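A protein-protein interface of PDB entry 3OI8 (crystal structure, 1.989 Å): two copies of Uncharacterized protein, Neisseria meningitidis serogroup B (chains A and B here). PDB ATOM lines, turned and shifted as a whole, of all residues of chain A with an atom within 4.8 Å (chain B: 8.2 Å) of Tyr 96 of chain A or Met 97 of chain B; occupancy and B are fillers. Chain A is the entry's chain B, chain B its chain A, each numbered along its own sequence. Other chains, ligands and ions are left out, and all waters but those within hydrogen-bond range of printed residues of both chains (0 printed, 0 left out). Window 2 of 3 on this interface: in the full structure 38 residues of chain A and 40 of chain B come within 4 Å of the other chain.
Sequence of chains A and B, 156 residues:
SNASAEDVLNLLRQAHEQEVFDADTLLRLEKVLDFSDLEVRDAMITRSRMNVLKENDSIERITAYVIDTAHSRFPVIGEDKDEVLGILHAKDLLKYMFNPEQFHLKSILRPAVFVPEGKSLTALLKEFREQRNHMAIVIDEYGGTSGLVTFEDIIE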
ATOM      1  N   ILE A  59     -19.686  24.156 -11.206  1.00  0.00           N
ATOM      2  CA  ILE A  59     -20.094  23.035 -10.347  1.00  0.00           C
ATOM      3  C   ILE A  59     -18.884  22.223  -9.877  1.00  0.00           C
ATOM      4  O   ILE A  59     -18.846  21.756  -8.738  1.00  0.00           O
ATOM      5  CB  ILE A  59     -21.144  22.122 -11.041  1.00  0.00           C
ATOM      6  CG1 ILE A  59     -21.705  21.084 -10.053  1.00  0.00           C
ATOM      7  CG2 ILE A  59     -20.554  21.452 -12.293  1.00  0.00           C
ATOM      8  CD1 ILE A  59     -22.199  21.697  -8.760  1.00  0.00           C
ATOM      9  N   THR A  63     -18.131  21.989  -5.969  1.00  0.00           N
ATOM     10  CA  THR A  63     -18.235  20.660  -5.371  1.00  0.00           C
ATOM     11  C   THR A  63     -16.931  20.263  -4.661  1.00  0.00           C
ATOM     12  O   THR A  63     -16.968  19.724  -3.575  1.00  0.00           O
ATOM     13  CB  THR A  63     -18.618  19.569  -6.416  1.00  0.00           C
ATOM     14  OG1 THR A  63     -19.886  19.898  -6.995  1.00  0.00           O
ATOM     15  CG2 THR A  63     -18.711  18.190  -5.740  1.00  0.00           C
ATOM     16  N   LEU A  93     -26.885  20.306  -3.401  1.00  0.00           N
ATOM     17  CA  LEU A  93     -26.149  20.064  -4.645  1.00  0.00           C
ATOM     18  C   LEU A  93     -26.496  18.718  -5.304  1.00  0.00           C
ATOM     19  O   LEU A  93     -26.261  18.527  -6.494  1.00  0.00           O
ATOM     20  CB  LEU A  93     -24.639  20.107  -4.395  1.00  0.00           C
ATOM     21  CG  LEU A  93     -23.942  21.454  -4.180  1.00  0.00           C
ATOM     22  CD1 LEU A  93     -22.512  21.225  -3.726  1.00  0.00           C
ATOM     23  CD2 LEU A  93     -23.976  22.316  -5.444  1.00  0.00           C
ATOM     24  N   LEU A  94     -27.011  17.782  -4.512  1.00  0.00           N
ATOM     25  CA  LEU A  94     -27.370  16.456  -4.997  1.00  0.00           C
ATOM     26  C   LEU A  94     -28.419  16.539  -6.097  1.00  0.00           C
ATOM     27  O   LEU A  94     -28.587  15.601  -6.907  1.00  0.00           O
ATOM     28  CB  LEU A  94     -27.893  15.598  -3.835  1.00  0.00           C
ATOM     29  CG  LEU A  94     -26.798  15.121  -2.867  1.00  0.00           C
ATOM     30  CD1 LEU A  94     -27.389  14.205  -1.806  1.00  0.00           C
ATOM     31  CD2 LEU A  94     -25.687  14.415  -3.668  1.00  0.00           C
ATOM     32  N   LYS A  95     -29.121  17.668  -6.117  1.00  0.00           N
ATOM     33  CA  LYS A  95     -30.139  17.930  -7.121  1.00  0.00           C
ATOM     34  C   LYS A  95     -29.560  17.826  -8.529  1.00  0.00           C
ATOM     35  O   LYS A  95     -30.278  17.526  -9.481  1.00  0.00           O
ATOM     36  CB  LYS A  95     -30.744  19.318  -6.900  1.00  0.00           C
ATOM     37  CG  LYS A  95     -31.717  19.750  -7.982  1.00  0.00           C
ATOM     38  CD  LYS A  95     -32.066  21.229  -7.845  1.00  0.00           C
ATOM     39  CE  LYS A  95     -33.041  21.673  -8.927  1.00  0.00           C
ATOM     40  NZ  LYS A  95     -33.418  23.103  -8.762  1.00  0.00           N
ATOM     41  N   TYR A  96     -28.256  18.064  -8.654  1.00  0.00           N
ATOM     42  CA  TYR A  96     -27.600  18.029  -9.961  1.00  0.00           C
ATOM     43  C   TYR A  96     -26.693  16.814 -10.190  1.00  0.00           C
ATOM     44  O   TYR A  96     -25.897  16.817 -11.119  1.00  0.00           O
ATOM     45  CB  TYR A  96     -26.812  19.322 -10.182  1.00  0.00           C
ATOM     46  CG  TYR A  96     -27.703  20.539 -10.187  1.00  0.00           C
ATOM     47  CD1 TYR A  96     -28.480  20.843 -11.303  1.00  0.00           C
ATOM     48  CD2 TYR A  96     -27.781  21.378  -9.077  1.00  0.00           C
ATOM     49  CE1 TYR A  96     -29.298  21.945 -11.315  1.00  0.00           C
ATOM     50  CE2 TYR A  96     -28.612  22.487  -9.075  1.00  0.00           C
ATOM     51  CZ  TYR A  96     -29.363  22.762 -10.203  1.00  0.00           C
ATOM     52  OH  TYR A  96     -30.189  23.853 -10.231  1.00  0.00           O
ATOM     53  N   MET A  97     -26.836  15.777  -9.364  1.00  0.00           N
ATOM     54  CA  MET A  97     -25.993  14.568  -9.467  1.00  0.00           C
ATOM     55  C   MET A  97     -25.910  13.935 -10.847  1.00  0.00           C
ATOM     56  O   MET A  97     -24.830  13.543 -11.300  1.00  0.00           O
ATOM     57  CB  MET A  97     -26.450  13.507  -8.472  1.00  0.00           C
ATOM     58  CG  MET A  97     -25.983  13.789  -7.064  1.00  0.00           C
ATOM     59  SD  MET A  97     -24.119  13.267  -6.807  1.00  0.00           S
ATOM     60  CE  MET A  97     -24.299  11.397  -7.290  1.00  0.00           C
ATOM     61  N   PHE A  98     -27.041  13.805 -11.519  1.00  0.00           N
ATOM     62  CA  PHE A  98     -27.016  13.149 -12.828  1.00  0.00           C
ATOM     63  C   PHE A  98     -27.327  14.112 -13.950  1.00  0.00           C
ATOM     64  O   PHE A  98     -27.690  13.715 -15.055  1.00  0.00           O
ATOM     65  CB  PHE A  98     -27.954  11.950 -12.824  1.00  0.00           C
ATOM     66  CG  PHE A  98     -27.742  11.066 -11.650  1.00  0.00           C
ATOM     67  CD1 PHE A  98     -26.711  10.141 -11.646  1.00  0.00           C
ATOM     68  CD2 PHE A  98     -28.527  11.200 -10.523  1.00  0.00           C
ATOM     69  CE1 PHE A  98     -26.492   9.342 -10.545  1.00  0.00           C
ATOM     70  CE2 PHE A  98     -28.311  10.406  -9.421  1.00  0.00           C
ATOM     71  CZ  PHE A  98     -27.285   9.481  -9.435  1.00  0.00           C
ATOM     72  N   ASN A  99     -27.168  15.392 -13.659  1.00  0.00           N
ATOM     73  CA  ASN A  99     -27.270  16.409 -14.695  1.00  0.00           C
ATOM     74  C   ASN A  99     -26.453  17.651 -14.321  1.00  0.00           C
ATOM     75  O   ASN A  99     -26.996  18.754 -14.269  1.00  0.00           O
ATOM     76  CB  ASN A  99     -28.744  16.763 -14.961  1.00  0.00           C
ATOM     77  CG  ASN A  99     -29.402  17.536 -13.802  1.00  0.00           C
ATOM     78  OD1 ASN A  99     -30.232  18.420 -14.025  1.00  0.00           O
ATOM     79  ND2 ASN A  99     -29.031  17.201 -12.569  1.00  0.00           N
ATOM     80  N   PRO A 100     -25.143  17.463 -14.061  1.00  0.00           N
ATOM     81  CA  PRO A 100     -24.226  18.534 -13.641  1.00  0.00           C
ATOM     82  C   PRO A 100     -24.191  19.683 -14.649  1.00  0.00           C
ATOM     83  O   PRO A 100     -23.871  20.800 -14.262  1.00  0.00           O
ATOM     84  CB  PRO A 100     -22.856  17.842 -13.594  1.00  0.00           C
ATOM     85  CG  PRO A 100     -23.137  16.390 -13.537  1.00  0.00           C
ATOM     86  CD  PRO A 100     -24.449  16.172 -14.221  1.00  0.00           C
ATOM     87  N   GLN A 102     -26.739  20.982 -16.005  1.00  0.00           N
ATOM     88  CA  GLN A 102     -27.872  21.846 -15.660  1.00  0.00           C
ATOM     89  C   GLN A 102     -27.623  22.741 -14.434  1.00  0.00           C
ATOM     90  O   GLN A 102     -28.524  23.457 -14.003  1.00  0.00           O
ATOM     91  CB  GLN A 102     -29.120  20.999 -15.376  1.00  0.00           C
ATOM     92  CG  GLN A 102     -30.137  20.943 -16.502  1.00  0.00           C
ATOM     93  CD  GLN A 102     -29.763  19.945 -17.572  1.00  0.00           C
ATOM     94  OE1 GLN A 102     -30.093  18.760 -17.475  1.00  0.00           O
ATOM     95  NE2 GLN A 102     -29.067  20.415 -18.599  1.00  0.00           N
ATOM     96  N   PHE A 103     -26.423  22.688 -13.863  1.00  0.00           N
ATOM     97  CA  PHE A 103     -26.148  23.392 -12.604  1.00  0.00           C
ATOM     98  C   PHE A 103     -26.552  24.855 -12.662  1.00  0.00           C
ATOM     99  O   PHE A 103     -26.132  25.591 -13.553  1.00  0.00           O
ATOM    100  CB  PHE A 103     -24.669  23.277 -12.232  1.00  0.00           C
ATOM    101  CG  PHE A 103     -24.301  23.973 -10.940  1.00  0.00           C
ATOM    102  CD1 PHE A 103     -24.899  23.608  -9.741  1.00  0.00           C
ATOM    103  CD2 PHE A 103     -23.334  24.973 -10.928  1.00  0.00           C
ATOM    104  CE1 PHE A 103     -24.550  24.238  -8.548  1.00  0.00           C
ATOM    105  CE2 PHE A 103     -22.972  25.603  -9.753  1.00  0.00           C
ATOM    106  CZ  PHE A 103     -23.585  25.238  -8.549  1.00  0.00           C
ATOM    107  N   HIS A 104     -27.371  25.269 -11.697  1.00  0.00           N
ATOM    108  CA  HIS A 104     -27.715  26.672 -11.505  1.00  0.00           C
ATOM    109  C   HIS A 104     -27.694  26.960  -9.996  1.00  0.00           C
ATOM    110  O   HIS A 104     -28.689  26.753  -9.304  1.00  0.00           O
ATOM    111  CB  HIS A 104     -29.094  26.952 -12.114  1.00  0.00           C
ATOM    112  CG  HIS A 104     -29.565  28.364 -11.947  1.00  0.00           C
ATOM    113  ND1 HIS A 104     -28.778  29.458 -12.241  1.00  0.00           N
ATOM    114  CD2 HIS A 104     -30.761  28.860 -11.549  1.00  0.00           C
ATOM    115  CE1 HIS A 104     -29.460  30.565 -12.007  1.00  0.00           C
ATOM    116  NE2 HIS A 104     -30.669  30.229 -11.589  1.00  0.00           N
ATOM    117  N   SER A 107     -30.583  28.570  -8.058  1.00  0.00           N
ATOM    118  CA  SER A 107     -31.849  27.884  -7.877  1.00  0.00           C
ATOM    119  C   SER A 107     -31.888  27.135  -6.542  1.00  0.00           C
ATOM    120  O   SER A 107     -32.957  26.726  -6.089  1.00  0.00           O
ATOM    121  CB  SER A 107     -32.096  26.909  -9.017  1.00  0.00           C
ATOM    122  OG  SER A 107     -31.345  25.727  -8.812  1.00  0.00           O
ATOM    123  N   ILE A 108     -30.730  26.938  -5.914  1.00  0.00           N
ATOM    124  CA  ILE A 108     -30.691  26.208  -4.636  1.00  0.00           C
ATOM    125  C   ILE A 108     -30.182  27.086  -3.492  1.00  0.00           C
ATOM    126  O   ILE A 108     -29.868  26.606  -2.407  1.00  0.00           O
ATOM    127  CB  ILE A 108     -29.848  24.917  -4.722  1.00  0.00           C
ATOM    128  CG1 ILE A 108     -28.427  25.226  -5.193  1.00  0.00           C
ATOM    129  CG2 ILE A 108     -30.515  23.890  -5.661  1.00  0.00           C
ATOM    130  CD1 ILE A 108     -27.496  24.004  -5.145  1.00  0.00           C
ATOM    131  N   ILE B  59     -26.756   4.022  -6.994  1.00  0.00           N
ATOM    132  CA  ILE B  59     -26.548   5.426  -6.678  1.00  0.00           C
ATOM    133  C   ILE B  59     -27.775   6.275  -7.038  1.00  0.00           C
ATOM    134  O   ILE B  59     -28.137   7.186  -6.302  1.00  0.00           O
ATOM    135  CB  ILE B  59     -25.251   5.987  -7.316  1.00  0.00           C
ATOM    136  CG1 ILE B  59     -24.962   7.387  -6.757  1.00  0.00           C
ATOM    137  CG2 ILE B  59     -25.314   5.945  -8.836  1.00  0.00           C
ATOM    138  CD1 ILE B  59     -23.545   7.850  -6.974  1.00  0.00           C
ATOM    139  N   THR B  63     -29.752   8.331  -4.234  1.00  0.00           N
ATOM    140  CA  THR B  63     -29.762   9.782  -4.351  1.00  0.00           C
ATOM    141  C   THR B  63     -31.189  10.348  -4.377  1.00  0.00           C
ATOM    142  O   THR B  63     -31.480  11.341  -3.709  1.00  0.00           O
ATOM    143  CB  THR B  63     -28.953  10.271  -5.583  1.00  0.00           C
ATOM    144  OG1 THR B  63     -27.567   9.949  -5.400  1.00  0.00           O
ATOM    145  CG2 THR B  63     -29.083  11.776  -5.741  1.00  0.00           C
ATOM    146  N   ILE B  67     -32.835  12.865  -1.513  1.00  0.00           N
ATOM    147  CA  ILE B  67     -33.410  14.161  -1.856  1.00  0.00           C
ATOM    148  C   ILE B  67     -34.869  14.242  -1.421  1.00  0.00           C
ATOM    149  O   ILE B  67     -35.310  15.241  -0.843  1.00  0.00           O
ATOM    150  CB  ILE B  67     -33.301  14.420  -3.359  1.00  0.00           C
ATOM    151  CG1 ILE B  67     -31.842  14.690  -3.734  1.00  0.00           C
ATOM    152  CG2 ILE B  67     -34.247  15.557  -3.794  1.00  0.00           C
ATOM    153  CD1 ILE B  67     -31.582  14.610  -5.224  1.00  0.00           C
ATOM    154  N   LYS B  91     -24.040  14.310   2.108  1.00  0.00           N
ATOM    155  CA  LYS B  91     -23.045  15.089   1.381  1.00  0.00           C
ATOM    156  C   LYS B  91     -21.795  14.294   1.008  1.00  0.00           C
ATOM    157  O   LYS B  91     -20.970  14.771   0.240  1.00  0.00           O
ATOM    158  CB  LYS B  91     -22.666  16.355   2.145  1.00  0.00           C
ATOM    159  CG  LYS B  91     -21.937  16.144   3.454  1.00  0.00           C
ATOM    160  CD  LYS B  91     -21.713  17.504   4.136  1.00  0.00           C
ATOM    161  CE  LYS B  91     -21.153  17.369   5.552  1.00  0.00           C
ATOM    162  NZ  LYS B  91     -19.715  16.964   5.568  1.00  0.00           N
ATOM    163  N   ASP B  92     -21.647  13.088   1.546  1.00  0.00           N
ATOM    164  CA  ASP B  92     -20.549  12.222   1.117  1.00  0.00           C
ATOM    165  C   ASP B  92     -20.820  11.669  -0.279  1.00  0.00           C
ATOM    166  O   ASP B  92     -19.897  11.249  -0.983  1.00  0.00           O
ATOM    167  CB  ASP B  92     -20.280  11.107   2.147  1.00  0.00           C
ATOM    168  CG  ASP B  92     -19.602  11.642   3.405  1.00  0.00           C
ATOM    169  OD1 ASP B  92     -19.029  12.752   3.327  1.00  0.00           O
ATOM    170  OD2 ASP B  92     -19.638  10.976   4.467  1.00  0.00           O
ATOM    171  N   LEU B  93     -22.087  11.693  -0.692  1.00  0.00           N
ATOM    172  CA  LEU B  93     -22.452  11.252  -2.034  1.00  0.00           C
ATOM    173  C   LEU B  93     -21.846  12.160  -3.124  1.00  0.00           C
ATOM    174  O   LEU B  93     -21.672  11.737  -4.267  1.00  0.00           O
ATOM    175  CB  LEU B  93     -23.972  11.203  -2.198  1.00  0.00           C
ATOM    176  CG  LEU B  93     -24.737  10.055  -1.523  1.00  0.00           C
ATOM    177  CD1 LEU B  93     -26.230  10.307  -1.660  1.00  0.00           C
ATOM    178  CD2 LEU B  93     -24.361   8.721  -2.159  1.00  0.00           C
ATOM    179  N   LEU B  94     -21.517  13.394  -2.766  1.00  0.00           N
ATOM    180  CA  LEU B  94     -21.020  14.348  -3.754  1.00  0.00           C
ATOM    181  C   LEU B  94     -19.648  13.924  -4.269  1.00  0.00           C
ATOM    182  O   LEU B  94     -19.178  14.417  -5.292  1.00  0.00           O
ATOM    183  CB  LEU B  94     -20.933  15.746  -3.153  1.00  0.00           C
ATOM    184  CG  LEU B  94     -22.249  16.424  -2.777  1.00  0.00           C
ATOM    185  CD1 LEU B  94     -21.949  17.727  -2.060  1.00  0.00           C
ATOM    186  CD2 LEU B  94     -23.107  16.665  -4.010  1.00  0.00           C
ATOM    187  N   LYS B  95     -18.997  13.025  -3.543  1.00  0.00           N
ATOM    188  CA  LYS B  95     -17.720  12.482  -3.996  1.00  0.00           C
ATOM    189  C   LYS B  95     -17.880  11.785  -5.348  1.00  0.00           C
ATOM    190  O   LYS B  95     -16.902  11.547  -6.057  1.00  0.00           O
ATOM    191  CB  LYS B  95     -17.155  11.495  -2.960  1.00  0.00           C
ATOM    192  CG  LYS B  95     -16.831  12.132  -1.607  1.00  0.00           C
ATOM    193  CD  LYS B  95     -16.310  11.102  -0.605  1.00  0.00           C
ATOM    194  CE  LYS B  95     -16.244  11.670   0.812  1.00  0.00           C
ATOM    195  NZ  LYS B  95     -16.158  10.599   1.864  1.00  0.00           N
ATOM    196  N   TYR B  96     -19.116  11.444  -5.700  1.00  0.00           N
ATOM    197  CA  TYR B  96     -19.357  10.692  -6.926  1.00  0.00           C
ATOM    198  C   TYR B  96     -20.111  11.520  -7.956  1.00  0.00           C
ATOM    199  O   TYR B  96     -20.699  10.979  -8.882  1.00  0.00           O
ATOM    200  CB  TYR B  96     -20.112   9.394  -6.626  1.00  0.00           C
ATOM    201  CG  TYR B  96     -19.278   8.390  -5.884  1.00  0.00           C
ATOM    202  CD1 TYR B  96     -18.209   7.756  -6.507  1.00  0.00           C
ATOM    203  CD2 TYR B  96     -19.557   8.071  -4.556  1.00  0.00           C
ATOM    204  CE1 TYR B  96     -17.436   6.832  -5.824  1.00  0.00           C
ATOM    205  CE2 TYR B  96     -18.789   7.156  -3.864  1.00  0.00           C
ATOM    206  CZ  TYR B  96     -17.736   6.535  -4.505  1.00  0.00           C
ATOM    207  OH  TYR B  96     -16.976   5.608  -3.824  1.00  0.00           O
ATOM    208  N   MET B  97     -20.093  12.836  -7.782  1.00  0.00           N
ATOM    209  CA  MET B  97     -20.802  13.739  -8.676  1.00  0.00           C
ATOM    210  C   MET B  97     -20.392  13.531 -10.133  1.00  0.00           C
ATOM    211  O   MET B  97     -21.235  13.511 -11.030  1.00  0.00           O
ATOM    212  CB  MET B  97     -20.527  15.183  -8.257  1.00  0.00           C
ATOM    213  CG  MET B  97     -20.922  16.243  -9.275  1.00  0.00           C
ATOM    214  SD  MET B  97     -22.702  16.971  -9.012  1.00  0.00           S
ATOM    215  CE  MET B  97     -22.949  16.518  -7.115  1.00  0.00           C
ATOM    216  N   PHE B  98     -19.100  13.359 -10.373  1.00  0.00           N
ATOM    217  CA  PHE B  98     -18.613  13.268 -11.750  1.00  0.00           C
ATOM    218  C   PHE B  98     -18.219  11.876 -12.218  1.00  0.00           C
ATOM    219  O   PHE B  98     -17.911  11.681 -13.398  1.00  0.00           O
ATOM    220  CB  PHE B  98     -17.486  14.276 -11.963  1.00  0.00           C
ATOM    221  CG  PHE B  98     -17.824  15.635 -11.431  1.00  0.00           C
ATOM    222  CD1 PHE B  98     -18.662  16.478 -12.141  1.00  0.00           C
ATOM    223  CD2 PHE B  98     -17.352  16.046 -10.194  1.00  0.00           C
ATOM    224  CE1 PHE B  98     -19.001  17.726 -11.643  1.00  0.00           C
ATOM    225  CE2 PHE B  98     -17.693  17.289  -9.689  1.00  0.00           C
ATOM    226  CZ  PHE B  98     -18.520  18.127 -10.416  1.00  0.00           C
ATOM    227  N   ASN B  99     -18.247  10.913 -11.302  1.00  0.00           N
ATOM    228  CA  ASN B  99     -17.953   9.519 -11.614  1.00  0.00           C
ATOM    229  C   ASN B  99     -18.942   8.603 -10.891  1.00  0.00           C
ATOM    230  O   ASN B  99     -18.538   7.809 -10.043  1.00  0.00           O
ATOM    231  CB  ASN B  99     -16.536   9.165 -11.158  1.00  0.00           C
ATOM    232  CG  ASN B  99     -16.317   9.448  -9.670  1.00  0.00           C
ATOM    233  OD1 ASN B  99     -17.053  10.226  -9.068  1.00  0.00           O
ATOM    234  ND2 ASN B  99     -15.320   8.808  -9.075  1.00  0.00           N
ATOM    235  N   PRO B 100     -20.241   8.715 -11.213  1.00  0.00           N
ATOM    236  CA  PRO B 100     -21.229   7.896 -10.492  1.00  0.00           C
ATOM    237  C   PRO B 100     -21.011   6.413 -10.763  1.00  0.00           C
ATOM    238  O   PRO B 100     -21.325   5.560  -9.928  1.00  0.00           O
ATOM    239  CB  PRO B 100     -22.574   8.345 -11.084  1.00  0.00           C
ATOM    240  CG  PRO B 100     -22.284   9.588 -11.864  1.00  0.00           C
ATOM    241  CD  PRO B 100     -20.855   9.506 -12.291  1.00  0.00           C
ATOM    242  N   GLU B 101     -20.457   6.111 -11.928  1.00  0.00           N
ATOM    243  CA  GLU B 101     -20.195   4.734 -12.306  1.00  0.00           C
ATOM    244  C   GLU B 101     -19.228   4.059 -11.336  1.00  0.00           C
ATOM    245  O   GLU B 101     -19.174   2.828 -11.253  1.00  0.00           O
ATOM    246  CB  GLU B 101     -19.711   4.648 -13.770  1.00  0.00           C
ATOM    247  CG  GLU B 101     -18.310   5.180 -14.049  1.00  0.00           C
ATOM    248  CD  GLU B 101     -18.204   6.705 -14.053  1.00  0.00           C
ATOM    249  OE1 GLU B 101     -19.242   7.401 -14.007  1.00  0.00           O
ATOM    250  OE2 GLU B 101     -17.064   7.210 -14.118  1.00  0.00           O
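The backbone carbonyl oxygen of Tyr 96 of chain A lies close to the side-chain amide nitrogen of Asn 99 of chain A (3.5 Å). The side-chain hydroxyl of Tyr 96 of chain A lies within hydrogen-bond range of the side-chain hydroxyl of Ser 107 of chain A, at 2.6 Å. OH of Tyr 96 of chain A sits at hydrogen-bond distance from O of His 104 of chain A. The backbone carbonyl oxygen (O) of Ile 59 of chain B sits at hydrogen-bond distance from the side-chain hydroxyl (OG1) of Thr 63 of chain B (3.0 Å). OG1 of Thr 63 of chain A is in hydrogen-bond range of O of Ile 59 of chain A (2.8 Å).
Of the printed residues of chain B, Tyr 96 of chain A touches Met 97. Met 97 of chain B touches just these residues of chain A: Leu 93, Tyr 96 and Met 97. No residue of chain B comes within 4 Å of Lys 95 of chain A. Printed residues of chain B within 4 Å of Met 97 of chain A: Ile 59, Thr 63, Leu 93, Tyr 96 and Met 97. Of the printed residues of chain B, Phe 98 of chain A touches Ile 59 (3.98 Å) and Thr 63 (3.9 Å). Of the printed residues of chain A, Leu 94 of chain B touches Thr 63, Leu 93 and Leu 94. Of the printed residues of chain B, Leu 93 of chain A touches Leu 94 and Met 97. Ser 107 of chain A touches none of the printed residues of chain B. The nearest residue of chain B that does not touch Tyr 96 of chain A is Ile 67 of chain B (5.9 Å). The nearest printed residue of chain A that does not touch Tyr 96 of chain B is Phe 98 of chain A (6.2 Å).
Thr 63 of chain A touches Leu 94 of chain B, but with the chains exchanged Leu 94 of chain A does not touch Thr 63 of chain B (4.03 Å). Leu 93 of chain A touches Leu 94 of chain B, and with the chains exchanged Leu 94 of chain A touches Leu 93 of chain B. Leu 94 of chain B touches its own counterpart, Leu 94 of chain A. Tyr 96 of chain A touches Met 97 of chain B, and with the chains exchanged Met 97 of chain A touches Tyr 96 of chain B. 10 positions are printed for both chains. Of the 14 pairs that touch across the chains among the printed residues, 8 have their exchanged pair printed and touching as well.
Of the 14 printed residues of chain B, 7 touch a printed residue of chain A. Hydrophobic or aromatic side chains of chain B within 4 Å of the printed part of chain A: Ile 59, Ile 67, Leu 93, Leu 94 and Met 97. Hydrophobic or aromatic side chains of chain A within 4 Å of the printed part of chain B: Leu 93, Leu 94, Met 97 and Phe 98. Among the printed residues, 14 pairs touch across the chains.
Leu 94 of chain B touches Leu 93 of chain A. CD1 of Ile 67 of chain B touches O of Leu 94 of chain A, 3.6 Å away. SD of Met 97 of chain B touches O of Tyr 96 of chain A, 3.8 Å away. Ile 59 of chain B touches Met 97 of chain A (CD1 to CE, 3.6 Å). CG2 of Thr 63 of chain B touches CG of Met 97 of chain A, 3.9 Å away. Leu 93 of chain B touches Met 97 of chain A (O to SD, 3.8 Å). O of Tyr 96 of chain B touches CE of Met 97 of chain A, 3.96 Å away. Met 97 of chain A touches Met 97 of chain B (SD to CE, 3.5 Å). Ile 59 of chain B touches Phe 98 of chain A. Phe 98 of chain A touches Thr 63 of chain B (CE2 to CB, 3.9 Å).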
